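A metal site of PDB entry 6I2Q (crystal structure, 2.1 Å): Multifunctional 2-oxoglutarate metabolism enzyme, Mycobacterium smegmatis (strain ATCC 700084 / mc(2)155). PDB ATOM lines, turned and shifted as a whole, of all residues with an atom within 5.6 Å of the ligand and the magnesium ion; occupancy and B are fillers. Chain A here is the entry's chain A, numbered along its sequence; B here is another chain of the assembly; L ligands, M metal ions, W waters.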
ATOM      1  N   HIS A 180      32.249 -14.411  19.659  1.00  0.00           N
ATOM      2  CA  HIS A 180      32.039 -13.200  20.476  1.00  0.00           C
ATOM      3  C   HIS A 180      30.820 -13.226  21.411  1.00  0.00           C
ATOM      4  O   HIS A 180      30.916 -12.653  22.493  1.00  0.00           O
ATOM      5  CB  HIS A 180      31.961 -11.922  19.602  1.00  0.00           C
ATOM      6  CG  HIS A 180      30.919 -11.983  18.518  1.00  0.00           C
ATOM      7  ND1 HIS A 180      29.653 -11.431  18.689  1.00  0.00           N
ATOM      8  CD2 HIS A 180      30.986 -12.520  17.276  1.00  0.00           C
ATOM      9  CE1 HIS A 180      29.010 -11.654  17.565  1.00  0.00           C
ATOM     10  NE2 HIS A 180      29.765 -12.316  16.682  1.00  0.00           N
ATOM     11  N   ARG A 181      29.703 -13.848  21.016  1.00  0.00           N
ATOM     12  CA  ARG A 181      28.468 -13.798  21.856  1.00  0.00           C
ATOM     13  C   ARG A 181      28.684 -14.279  23.310  1.00  0.00           C
ATOM     14  O   ARG A 181      29.065 -15.418  23.545  1.00  0.00           O
ATOM     15  CB  ARG A 181      27.279 -14.563  21.223  1.00  0.00           C
ATOM     16  CG  ARG A 181      25.999 -14.356  22.030  1.00  0.00           C
ATOM     17  CD  ARG A 181      24.782 -14.964  21.389  1.00  0.00           C
ATOM     18  NE  ARG A 181      24.657 -14.606  19.975  1.00  0.00           N
ATOM     19  CZ  ARG A 181      24.181 -13.448  19.515  1.00  0.00           C
ATOM     20  NH1 ARG A 181      23.797 -12.494  20.366  1.00  0.00           N
ATOM     21  NH2 ARG A 181      24.089 -13.238  18.216  1.00  0.00           N
ATOM     22  N   SER A 245      37.227 -12.732  13.857  1.00  0.00           N
ATOM     23  CA  SER A 245      35.762 -12.702  13.737  1.00  0.00           C
ATOM     24  C   SER A 245      35.291 -13.904  12.915  1.00  0.00           C
ATOM     25  O   SER A 245      34.117 -14.253  12.999  1.00  0.00           O
ATOM     26  CB  SER A 245      35.283 -11.393  13.105  1.00  0.00           C
ATOM     27  OG  SER A 245      35.614 -10.320  13.967  1.00  0.00           O
ATOM     28  N   HIS A 246      36.206 -14.522  12.130  1.00  0.00           N
ATOM     29  CA  HIS A 246      35.880 -15.689  11.308  1.00  0.00           C
ATOM     30  C   HIS A 246      35.409 -16.833  12.202  1.00  0.00           C
ATOM     31  O   HIS A 246      36.207 -17.492  12.856  1.00  0.00           O
ATOM     32  CB  HIS A 246      37.103 -16.120  10.455  1.00  0.00           C
ATOM     33  CG  HIS A 246      37.563 -15.058   9.491  1.00  0.00           C
ATOM     34  ND1 HIS A 246      37.644 -15.305   8.134  1.00  0.00           N
ATOM     35  CD2 HIS A 246      37.857 -13.761   9.723  1.00  0.00           C
ATOM     36  CE1 HIS A 246      38.029 -14.165   7.590  1.00  0.00           C
ATOM     37  NE2 HIS A 246      38.169 -13.201   8.506  1.00  0.00           N
ATOM     38  N   LEU A 247      34.092 -17.038  12.234  1.00  0.00           N
ATOM     39  CA  LEU A 247      33.426 -18.064  13.050  1.00  0.00           C
ATOM     40  C   LEU A 247      33.976 -19.449  12.707  1.00  0.00           C
ATOM     41  O   LEU A 247      34.175 -19.777  11.543  1.00  0.00           O
ATOM     42  CB  LEU A 247      31.899 -18.008  12.828  1.00  0.00           C
ATOM     43  CG  LEU A 247      31.216 -16.651  13.177  1.00  0.00           C
ATOM     44  CD1 LEU A 247      29.757 -16.591  12.629  1.00  0.00           C
ATOM     45  CD2 LEU A 247      31.260 -16.377  14.680  1.00  0.00           C
ATOM     46  N   GLY A 285      27.978 -21.304  17.450  1.00  0.00           N
ATOM     47  CA  GLY A 285      26.644 -20.809  17.095  1.00  0.00           C
ATOM     48  C   GLY A 285      25.995 -21.858  16.209  1.00  0.00           C
ATOM     49  O   GLY A 285      26.694 -22.685  15.623  1.00  0.00           O
ATOM     50  N   ASP A 286      24.669 -21.865  16.101  1.00  0.00           N
ATOM     51  CA  ASP A 286      23.978 -22.906  15.329  1.00  0.00           C
ATOM     52  C   ASP A 286      24.177 -22.799  13.825  1.00  0.00           C
ATOM     53  O   ASP A 286      24.345 -23.842  13.191  1.00  0.00           O
ATOM     54  CB  ASP A 286      22.467 -22.935  15.651  1.00  0.00           C
ATOM     55  CG  ASP A 286      21.761 -21.576  15.553  1.00  0.00           C
ATOM     56  OD1 ASP A 286      22.204 -20.643  16.234  1.00  0.00           O
ATOM     57  OD2 ASP A 286      20.767 -21.471  14.797  1.00  0.00           O
ATOM     58  N   ALA A 287      24.136 -21.585  13.238  1.00  0.00           N
ATOM     59  CA  ALA A 287      24.323 -21.445  11.780  1.00  0.00           C
ATOM     60  C   ALA A 287      25.754 -21.778  11.348  1.00  0.00           C
ATOM     61  O   ALA A 287      25.910 -22.521  10.387  1.00  0.00           O
ATOM     62  CB  ALA A 287      23.940 -20.052  11.305  1.00  0.00           C
ATOM     63  N   ALA A 288      26.785 -21.266  12.076  1.00  0.00           N
ATOM     64  CA  ALA A 288      28.204 -21.499  11.744  1.00  0.00           C
ATOM     65  C   ALA A 288      28.613 -22.954  11.942  1.00  0.00           C
ATOM     66  O   ALA A 288      29.454 -23.454  11.191  1.00  0.00           O
ATOM     67  CB  ALA A 288      29.089 -20.619  12.616  1.00  0.00           C
ATOM     68  N   PHE A 289      28.038 -23.651  12.957  1.00  0.00           N
ATOM     69  CA  PHE A 289      28.406 -25.041  13.248  1.00  0.00           C
ATOM     70  C   PHE A 289      28.050 -25.963  12.070  1.00  0.00           C
ATOM     71  O   PHE A 289      28.809 -26.904  11.765  1.00  0.00           O
ATOM     72  CB  PHE A 289      27.770 -25.535  14.571  1.00  0.00           C
ATOM     73  CG  PHE A 289      28.423 -26.790  15.122  1.00  0.00           C
ATOM     74  CD1 PHE A 289      29.752 -26.792  15.521  1.00  0.00           C
ATOM     75  CD2 PHE A 289      27.685 -27.965  15.275  1.00  0.00           C
ATOM     76  CE1 PHE A 289      30.336 -27.934  16.077  1.00  0.00           C
ATOM     77  CE2 PHE A 289      28.281 -29.121  15.823  1.00  0.00           C
ATOM     78  CZ  PHE A 289      29.610 -29.101  16.210  1.00  0.00           C
ATOM     79  N   GLN A 292      30.288 -24.061   8.313  1.00  0.00           N
ATOM     80  CA  GLN A 292      31.739 -23.949   8.146  1.00  0.00           C
ATOM     81  C   GLN A 292      32.436 -25.326   8.054  1.00  0.00           C
ATOM     82  O   GLN A 292      32.444 -26.071   9.029  1.00  0.00           O
ATOM     83  CB  GLN A 292      32.303 -23.120   9.334  1.00  0.00           C
ATOM     84  CG  GLN A 292      31.897 -21.607   9.257  1.00  0.00           C
ATOM     85  CD  GLN A 292      32.584 -20.909   8.093  1.00  0.00           C
ATOM     86  OE1 GLN A 292      33.788 -20.952   7.931  1.00  0.00           O
ATOM     87  NE2 GLN A 292      31.829 -20.241   7.251  1.00  0.00           N
ATOM     88  N   VAL A 317      25.459 -22.779  21.194  1.00  0.00           N
ATOM     89  CA  VAL A 317      24.490 -21.812  21.682  1.00  0.00           C
ATOM     90  C   VAL A 317      23.467 -21.722  20.544  1.00  0.00           C
ATOM     91  O   VAL A 317      23.678 -21.018  19.538  1.00  0.00           O
ATOM     92  CB  VAL A 317      25.158 -20.454  22.086  1.00  0.00           C
ATOM     93  CG1 VAL A 317      24.104 -19.412  22.503  1.00  0.00           C
ATOM     94  CG2 VAL A 317      26.188 -20.678  23.212  1.00  0.00           C
ATOM     95  N   ASN A 318      22.453 -22.574  20.625  1.00  0.00           N
ATOM     96  CA  ASN A 318      21.486 -22.707  19.546  1.00  0.00           C
ATOM     97  C   ASN A 318      20.272 -21.811  19.773  1.00  0.00           C
ATOM     98  O   ASN A 318      19.236 -22.241  20.305  1.00  0.00           O
ATOM     99  CB  ASN A 318      21.104 -24.176  19.353  1.00  0.00           C
ATOM    100  CG  ASN A 318      20.130 -24.434  18.234  1.00  0.00           C
ATOM    101  OD1 ASN A 318      19.797 -23.542  17.443  1.00  0.00           O
ATOM    102  ND2 ASN A 318      19.679 -25.659  18.114  1.00  0.00           N
ATOM    103  N   ASN A 319      20.385 -20.560  19.289  1.00  0.00           N
ATOM    104  CA  ASN A 319      19.335 -19.553  19.422  1.00  0.00           C
ATOM    105  C   ASN A 319      18.387 -19.574  18.238  1.00  0.00           C
ATOM    106  O   ASN A 319      17.565 -18.672  18.087  1.00  0.00           O
ATOM    107  CB  ASN A 319      19.924 -18.156  19.638  1.00  0.00           C
ATOM    108  CG  ASN A 319      20.972 -17.759  18.647  1.00  0.00           C
ATOM    109  OD1 ASN A 319      21.101 -18.323  17.532  1.00  0.00           O
ATOM    110  ND2 ASN A 319      21.760 -16.790  19.044  1.00  0.00           N
ATOM    111  N   GLN A 320      18.476 -20.620  17.391  1.00  0.00           N
ATOM    112  CA  GLN A 320      17.566 -20.935  16.287  1.00  0.00           C
ATOM    113  C   GLN A 320      17.462 -19.783  15.255  1.00  0.00           C
ATOM    114  O   GLN A 320      16.402 -19.573  14.659  1.00  0.00           O
ATOM    115  CB  GLN A 320      16.189 -21.311  16.874  1.00  0.00           C
ATOM    116  CG  GLN A 320      16.333 -22.343  18.044  1.00  0.00           C
ATOM    117  CD  GLN A 320      15.024 -22.570  18.763  1.00  0.00           C
ATOM    118  OE1 GLN A 320      14.077 -23.112  18.194  1.00  0.00           O
ATOM    119  NE2 GLN A 320      14.955 -22.149  20.047  1.00  0.00           N
ATOM    120  N   ILE A 321      18.575 -19.073  15.050  1.00  0.00           N
ATOM    121  CA  ILE A 321      18.705 -17.927  14.135  1.00  0.00           C
ATOM    122  C   ILE A 321      20.205 -17.703  13.856  1.00  0.00           C
ATOM    123  O   ILE A 321      21.048 -18.066  14.678  1.00  0.00           O
ATOM    124  CB  ILE A 321      17.996 -16.654  14.716  1.00  0.00           C
ATOM    125  CG1 ILE A 321      17.817 -15.561  13.610  1.00  0.00           C
ATOM    126  CG2 ILE A 321      18.679 -16.100  16.014  1.00  0.00           C
ATOM    127  CD1 ILE A 321      16.805 -14.408  13.931  1.00  0.00           C
ATOM    128  N   GLY A 322      20.510 -17.118  12.705  1.00  0.00           N
ATOM    129  CA  GLY A 322      21.845 -16.745  12.293  1.00  0.00           C
ATOM    130  C   GLY A 322      21.707 -15.399  11.623  1.00  0.00           C
ATOM    131  O   GLY A 322      21.423 -15.342  10.424  1.00  0.00           O
ATOM    132  N   PHE A 323      21.872 -14.323  12.418  1.00  0.00           N
ATOM    133  CA  PHE A 323      21.696 -12.920  12.019  1.00  0.00           C
ATOM    134  C   PHE A 323      20.189 -12.748  11.619  1.00  0.00           C
ATOM    135  O   PHE A 323      19.351 -12.688  12.515  1.00  0.00           O
ATOM    136  CB  PHE A 323      22.710 -12.461  10.933  1.00  0.00           C
ATOM    137  CG  PHE A 323      22.861 -10.961  10.679  1.00  0.00           C
ATOM    138  CD1 PHE A 323      21.849 -10.071  11.023  1.00  0.00           C
ATOM    139  CD2 PHE A 323      24.003 -10.449  10.067  1.00  0.00           C
ATOM    140  CE1 PHE A 323      21.999  -8.693  10.799  1.00  0.00           C
ATOM    141  CE2 PHE A 323      24.142  -9.070   9.827  1.00  0.00           C
ATOM    142  CZ  PHE A 323      23.146  -8.203  10.207  1.00  0.00           C
ATOM    143  N   ARG A 384      17.614 -15.501  21.043  1.00  0.00           N
ATOM    144  CA  ARG A 384      18.380 -14.280  20.971  1.00  0.00           C
ATOM    145  C   ARG A 384      17.420 -13.140  21.268  1.00  0.00           C
ATOM    146  O   ARG A 384      16.653 -12.745  20.383  1.00  0.00           O
ATOM    147  CB  ARG A 384      19.057 -14.180  19.587  1.00  0.00           C
ATOM    148  CG  ARG A 384      20.180 -13.151  19.514  1.00  0.00           C
ATOM    149  CD  ARG A 384      20.455 -12.777  18.057  1.00  0.00           C
ATOM    150  NE  ARG A 384      19.327 -12.051  17.475  1.00  0.00           N
ATOM    151  CZ  ARG A 384      19.067 -11.967  16.176  1.00  0.00           C
ATOM    152  NH1 ARG A 384      19.869 -12.545  15.289  1.00  0.00           N
ATOM    153  NH2 ARG A 384      18.012 -11.291  15.747  1.00  0.00           N
ATOM    154  N   HIS A 388      20.331  -8.608  15.949  1.00  0.00           N
ATOM    155  CA  HIS A 388      21.719  -8.982  15.752  1.00  0.00           C
ATOM    156  C   HIS A 388      22.697  -7.874  16.183  1.00  0.00           C
ATOM    157  O   HIS A 388      23.763  -8.200  16.695  1.00  0.00           O
ATOM    158  CB  HIS A 388      21.985  -9.389  14.319  1.00  0.00           C
ATOM    159  CG  HIS A 388      23.314 -10.040  14.135  1.00  0.00           C
ATOM    160  ND1 HIS A 388      23.537 -11.357  14.531  1.00  0.00           N
ATOM    161  CD2 HIS A 388      24.454  -9.546  13.596  1.00  0.00           C
ATOM    162  CE1 HIS A 388      24.782 -11.631  14.193  1.00  0.00           C
ATOM    163  NE2 HIS A 388      25.387 -10.562  13.641  1.00  0.00           N
ATOM    164  N   GLN B 542      25.220 -14.099   2.593  1.00  0.00           N
ATOM    165  CA  GLN B 542      24.757 -14.080   3.981  1.00  0.00           C
ATOM    166  C   GLN B 542      23.907 -12.853   4.243  1.00  0.00           C
ATOM    167  O   GLN B 542      24.346 -11.703   4.028  1.00  0.00           O
ATOM    168  CB  GLN B 542      25.927 -14.190   4.956  1.00  0.00           C
ATOM    169  CG  GLN B 542      26.518 -15.609   4.996  1.00  0.00           C
ATOM    170  CD  GLN B 542      27.986 -15.608   5.322  1.00  0.00           C
ATOM    171  OE1 GLN B 542      28.505 -14.671   5.939  1.00  0.00           O
ATOM    172  NE2 GLN B 542      28.716 -16.635   4.910  1.00  0.00           N
ATOM    173  N   ASP B 543      22.643 -13.127   4.637  1.00  0.00           N
ATOM    174  CA  ASP B 543      21.572 -12.164   4.951  1.00  0.00           C
ATOM    175  C   ASP B 543      21.336 -11.182   3.782  1.00  0.00           C
ATOM    176  O   ASP B 543      20.938 -10.038   3.996  1.00  0.00           O
ATOM    177  CB  ASP B 543      21.937 -11.435   6.283  1.00  0.00           C
ATOM    178  CG  ASP B 543      22.232 -12.451   7.398  1.00  0.00           C
ATOM    179  OD1 ASP B 543      21.277 -13.050   7.914  1.00  0.00           O
ATOM    180  OD2 ASP B 543      23.434 -12.653   7.715  1.00  0.00           O
ATOM    181  N   LEU B 591      25.781 -20.449   6.165  1.00  0.00           N
ATOM    182  CA  LEU B 591      26.925 -19.679   6.683  1.00  0.00           C
ATOM    183  C   LEU B 591      28.211 -20.357   6.211  1.00  0.00           C
ATOM    184  O   LEU B 591      28.932 -21.001   6.992  1.00  0.00           O
ATOM    185  CB  LEU B 591      26.858 -19.569   8.230  1.00  0.00           C
ATOM    186  CG  LEU B 591      27.459 -18.300   8.844  1.00  0.00           C
ATOM    187  CD1 LEU B 591      27.018 -18.156  10.298  1.00  0.00           C
ATOM    188  CD2 LEU B 591      29.020 -18.267   8.720  1.00  0.00           C
ATOM    189  N   GLU B 593      31.472 -19.843   2.950  1.00  0.00           N
ATOM    190  CA  GLU B 593      32.111 -18.990   1.936  1.00  0.00           C
ATOM    191  C   GLU B 593      32.609 -19.917   0.827  1.00  0.00           C
ATOM    192  O   GLU B 593      32.261 -19.728  -0.321  1.00  0.00           O
ATOM    193  CB  GLU B 593      33.243 -18.094   2.494  1.00  0.00           C
ATOM    194  CG  GLU B 593      32.704 -16.917   3.293  1.00  0.00           C
ATOM    195  CD  GLU B 593      32.372 -17.220   4.744  1.00  0.00           C
ATOM    196  OE1 GLU B 593      31.564 -16.463   5.317  1.00  0.00           O
ATOM    197  OE2 GLU B 593      32.911 -18.193   5.317  1.00  0.00           O
ATOM    198  N   GLN B 617      29.423 -11.114   3.592  1.00  0.00           N
ATOM    199  CA  GLN B 617      28.816 -10.299   4.661  1.00  0.00           C
ATOM    200  C   GLN B 617      29.654  -9.019   4.797  1.00  0.00           C
ATOM    201  O   GLN B 617      29.131  -7.906   4.804  1.00  0.00           O
ATOM    202  CB  GLN B 617      28.727 -11.098   5.979  1.00  0.00           C
ATOM    203  CG  GLN B 617      27.992 -10.305   7.074  1.00  0.00           C
ATOM    204  CD  GLN B 617      26.771 -10.995   7.585  1.00  0.00           C
ATOM    205  OE1 GLN B 617      26.773 -11.582   8.646  1.00  0.00           O
ATOM    206  NE2 GLN B 617      25.690 -10.892   6.877  1.00  0.00           N
ATOM    207  N   PHE B 621      35.697 -11.826   4.935  1.00  0.00           N
ATOM    208  CA  PHE B 621      35.455 -13.250   5.085  1.00  0.00           C
ATOM    209  C   PHE B 621      35.574 -14.022   3.758  1.00  0.00           C
ATOM    210  O   PHE B 621      35.479 -15.254   3.757  1.00  0.00           O
ATOM    211  CB  PHE B 621      34.071 -13.502   5.744  1.00  0.00           C
ATOM    212  CG  PHE B 621      33.894 -12.771   7.060  1.00  0.00           C
ATOM    213  CD1 PHE B 621      32.936 -11.750   7.203  1.00  0.00           C
ATOM    214  CD2 PHE B 621      34.686 -13.078   8.163  1.00  0.00           C
ATOM    215  CE1 PHE B 621      32.777 -11.077   8.406  1.00  0.00           C
ATOM    216  CE2 PHE B 621      34.533 -12.391   9.374  1.00  0.00           C
ATOM    217  CZ  PHE B 621      33.587 -11.391   9.496  1.00  0.00           C
ATOM    218  N   HIS B 661      36.577  -6.338   9.595  1.00  0.00           N
ATOM    219  CA  HIS B 661      35.413  -5.569   9.150  1.00  0.00           C
ATOM    220  C   HIS B 661      35.876  -4.340   8.387  1.00  0.00           C
ATOM    221  O   HIS B 661      35.271  -3.283   8.508  1.00  0.00           O
ATOM    222  CB  HIS B 661      34.526  -5.186  10.364  1.00  0.00           C
ATOM    223  CG  HIS B 661      33.942  -6.395  11.028  1.00  0.00           C
ATOM    224  ND1 HIS B 661      34.632  -7.078  12.011  1.00  0.00           N
ATOM    225  CD2 HIS B 661      32.819  -7.078  10.719  1.00  0.00           C
ATOM    226  CE1 HIS B 661      33.886  -8.120  12.310  1.00  0.00           C
ATOM    227  NE2 HIS B 661      32.782  -8.156  11.561  1.00  0.00           N
HETATM  228  N1  LIG L   1      31.519 -15.722   7.915  1.00  0.00           N
HETATM  229  C1  LIG L   1      32.418 -16.022   8.872  1.00  0.00           C
HETATM  230  C2  LIG L   1      33.331 -17.171   8.619  1.00  0.00           C
HETATM  231  N2  LIG L   1      32.549 -15.368  10.033  1.00  0.00           N
HETATM  232  C3  LIG L   1      31.699 -14.347  10.296  1.00  0.00           C
HETATM  233  N3  LIG L   1      31.916 -13.649  11.411  1.00  0.00           N
HETATM  234  C4  LIG L   1      30.673 -13.991   9.356  1.00  0.00           C
HETATM  235  C5  LIG L   1      30.675 -14.715   8.186  1.00  0.00           C
HETATM  236  C6  LIG L   1      29.644 -12.927   9.611  1.00  0.00           C
HETATM  237  N4  LIG L   1      28.688 -13.266  10.701  1.00  0.00           N
HETATM  238  C7  LIG L   1      28.753 -12.742  11.911  1.00  0.00           C
HETATM  239  S1  LIG L   1      27.520 -13.275  12.913  1.00  0.00           S
HETATM  240  C8  LIG L   1      26.871 -14.248  11.655  1.00  0.00           C
HETATM  241  C9  LIG L   1      27.602 -14.125  10.514  1.00  0.00           C
HETATM  242  C10 LIG L   1      27.295 -14.720   9.187  1.00  0.00           C
HETATM  243  C11 LIG L   1      25.739 -15.197  11.957  1.00  0.00           C
HETATM  244  C12 LIG L   1      26.091 -16.142  13.086  1.00  0.00           C
HETATM  245  O1  LIG L   1      25.041 -17.119  13.245  1.00  0.00           O
HETATM  246  P1  LIG L   1      25.237 -18.271  14.397  1.00  0.00           P
HETATM  247  O2  LIG L   1      23.859 -18.958  14.579  1.00  0.00           O
HETATM  248  O3  LIG L   1      26.446 -19.043  14.107  1.00  0.00           O
HETATM  249  O4  LIG L   1      25.510 -17.412  15.701  1.00  0.00           O
HETATM  250  P2  LIG L   1      24.751 -16.295  16.551  1.00  0.00           P
HETATM  251  O5  LIG L   1      23.234 -16.523  16.355  1.00  0.00           O
HETATM  252  O6  LIG L   1      25.175 -14.928  16.138  1.00  0.00           O
HETATM  253  O7  LIG L   1      25.077 -16.648  17.997  1.00  0.00           O
HETATM  254 MG    MG M   1      22.557 -18.660  16.086  1.00  0.00          MG
HETATM  255  O   HOH W   1      28.631 -18.545  15.728  1.00  0.00           O
HETATM  256  O   HOH W   2      27.641  -9.822  10.950  1.00  0.00           O
HETATM  257  O   HOH W   3      23.816 -19.056  17.787  1.00  0.00           O
HETATM  258  O   HOH W   4      22.187 -14.250  15.194  1.00  0.00           O
HETATM  259  O   HOH W   5      27.617 -17.518  18.304  1.00  0.00           O
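Three residues have an atom within 4 Å of the magnesium ion: Asp 286, Asn 319 and Ile 321.
O2 of the ligand binds the magnesium ion (2.0 Å). The magnesium ion is bound by OD1 of Asp 286, at 2.0 Å. The magnesium ion is bound by OD1 of Asn 319. The backbone carbonyl oxygen (O) of Ile 321 binds the magnesium ion (2.1 Å). Water W3 binds the magnesium ion, 2.2 Å away. The magnesium ion is bound by O5 of the ligand (2.3 Å). The magnesium ion has six donor atoms within binding distance.
A nitrogen (N3) of the ligand sits at hydrogen-bond distance from the backbone carbonyl oxygen of Ser 245 (2.8 Å). The guanidinium group of Arg 181 lies within salt-bridge range of an oxygen (O7) of the ligand. A ring nitrogen (NE2) of His 388 sits close to a sulfur (S1) of the ligand (3.5 Å). An oxygen (O2) of the ligand lies close to the backbone NH of Ala 287 (3.0 Å). N of Leu 247 is in hydrogen-bond range of N2 of the ligand (3.2 Å). An oxygen (O3) of the ligand is in hydrogen-bond range of the backbone NH (N) of Ala 288. A nitrogen (N1) of the ligand is in hydrogen-bond range of the side-chain carboxylate (OE1) of Glu 593 of chain B (2.7 Å). O2 of the ligand lies close to N of Asp 286.
The side-chain amide nitrogen (NE2) of Gln 617 of chain B lies within hydrogen-bond range of the backbone carbonyl oxygen (O) of Gln 542 of chain B (3.3 Å). The side-chain carboxylate (OE1) of Glu 593 of chain B sits at hydrogen-bond distance from the side-chain amide nitrogen (NE2) of Gln 542 of chain B. OE2 of Glu 593 of chain B is in hydrogen-bond range of NE2 of Gln 292, 3.0 Å away. The side-chain amide nitrogen of Gln 292 is in hydrogen-bond range of the backbone carbonyl oxygen of Leu 591 of chain B (3.0 Å). The guanidinium group (NH1) of Arg 384 is in hydrogen-bond range of the backbone carbonyl oxygen (O) of Phe 323, 2.8 Å away. OD1 of Asn 318 sits close to OD2 of Asp 286, at 3.5 Å. OD2 of Asp 543 of chain B lies within hydrogen-bond range of NE2 of Gln 617 of chain B (3.0 Å).
Water W3 lies within hydrogen-bond range of the backbone carbonyl oxygen (O) of Val 317 (2.6 Å), an oxygen (O7) of the ligand (2.7 Å), the side-chain amide nitrogen (ND2) of Asn 319 (3.3 Å) and the backbone NH (N) of Asp 286 (3.4 Å). Water W4 lies within hydrogen-bond range of N of Phe 323 (2.8 Å), NH1 of Arg 384 (2.9 Å), O6 of the ligand (3.2 Å) and ND1 of His 388 (3.3 Å). Water W1 bridges O3 of the ligand and N of Gly 285.
A nitrogen (N4) of the ligand sits close to the side-chain amide oxygen (OE1) of Gln 617 of chain B, 3.3 Å away. Merely in contact with the ligand: His 246, Gly 285, Gln 292, Gly 322, Phe 323, Gln 542 of chain B, Leu 591 of chain B and Phe 621 of chain B. Hydrophobic or aromatic side chains that line the ligand: Leu 247, Ala 287, Ala 288, His 388, Leu 591 of chain B and Phe 621 of chain B. Within 4 Å of the ligand: Arg 181, Ser 245, His 246, Leu 247, Gly 285, Asp 286, Ala 287, Ala 288, Gln 292, Asn 319, Ile 321, Gly 322, Phe 323, His 388, Gln 542 of chain B, Leu 591 of chain B, Glu 593 of chain B, Gln 617 of chain B and Phe 621 of chain B.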
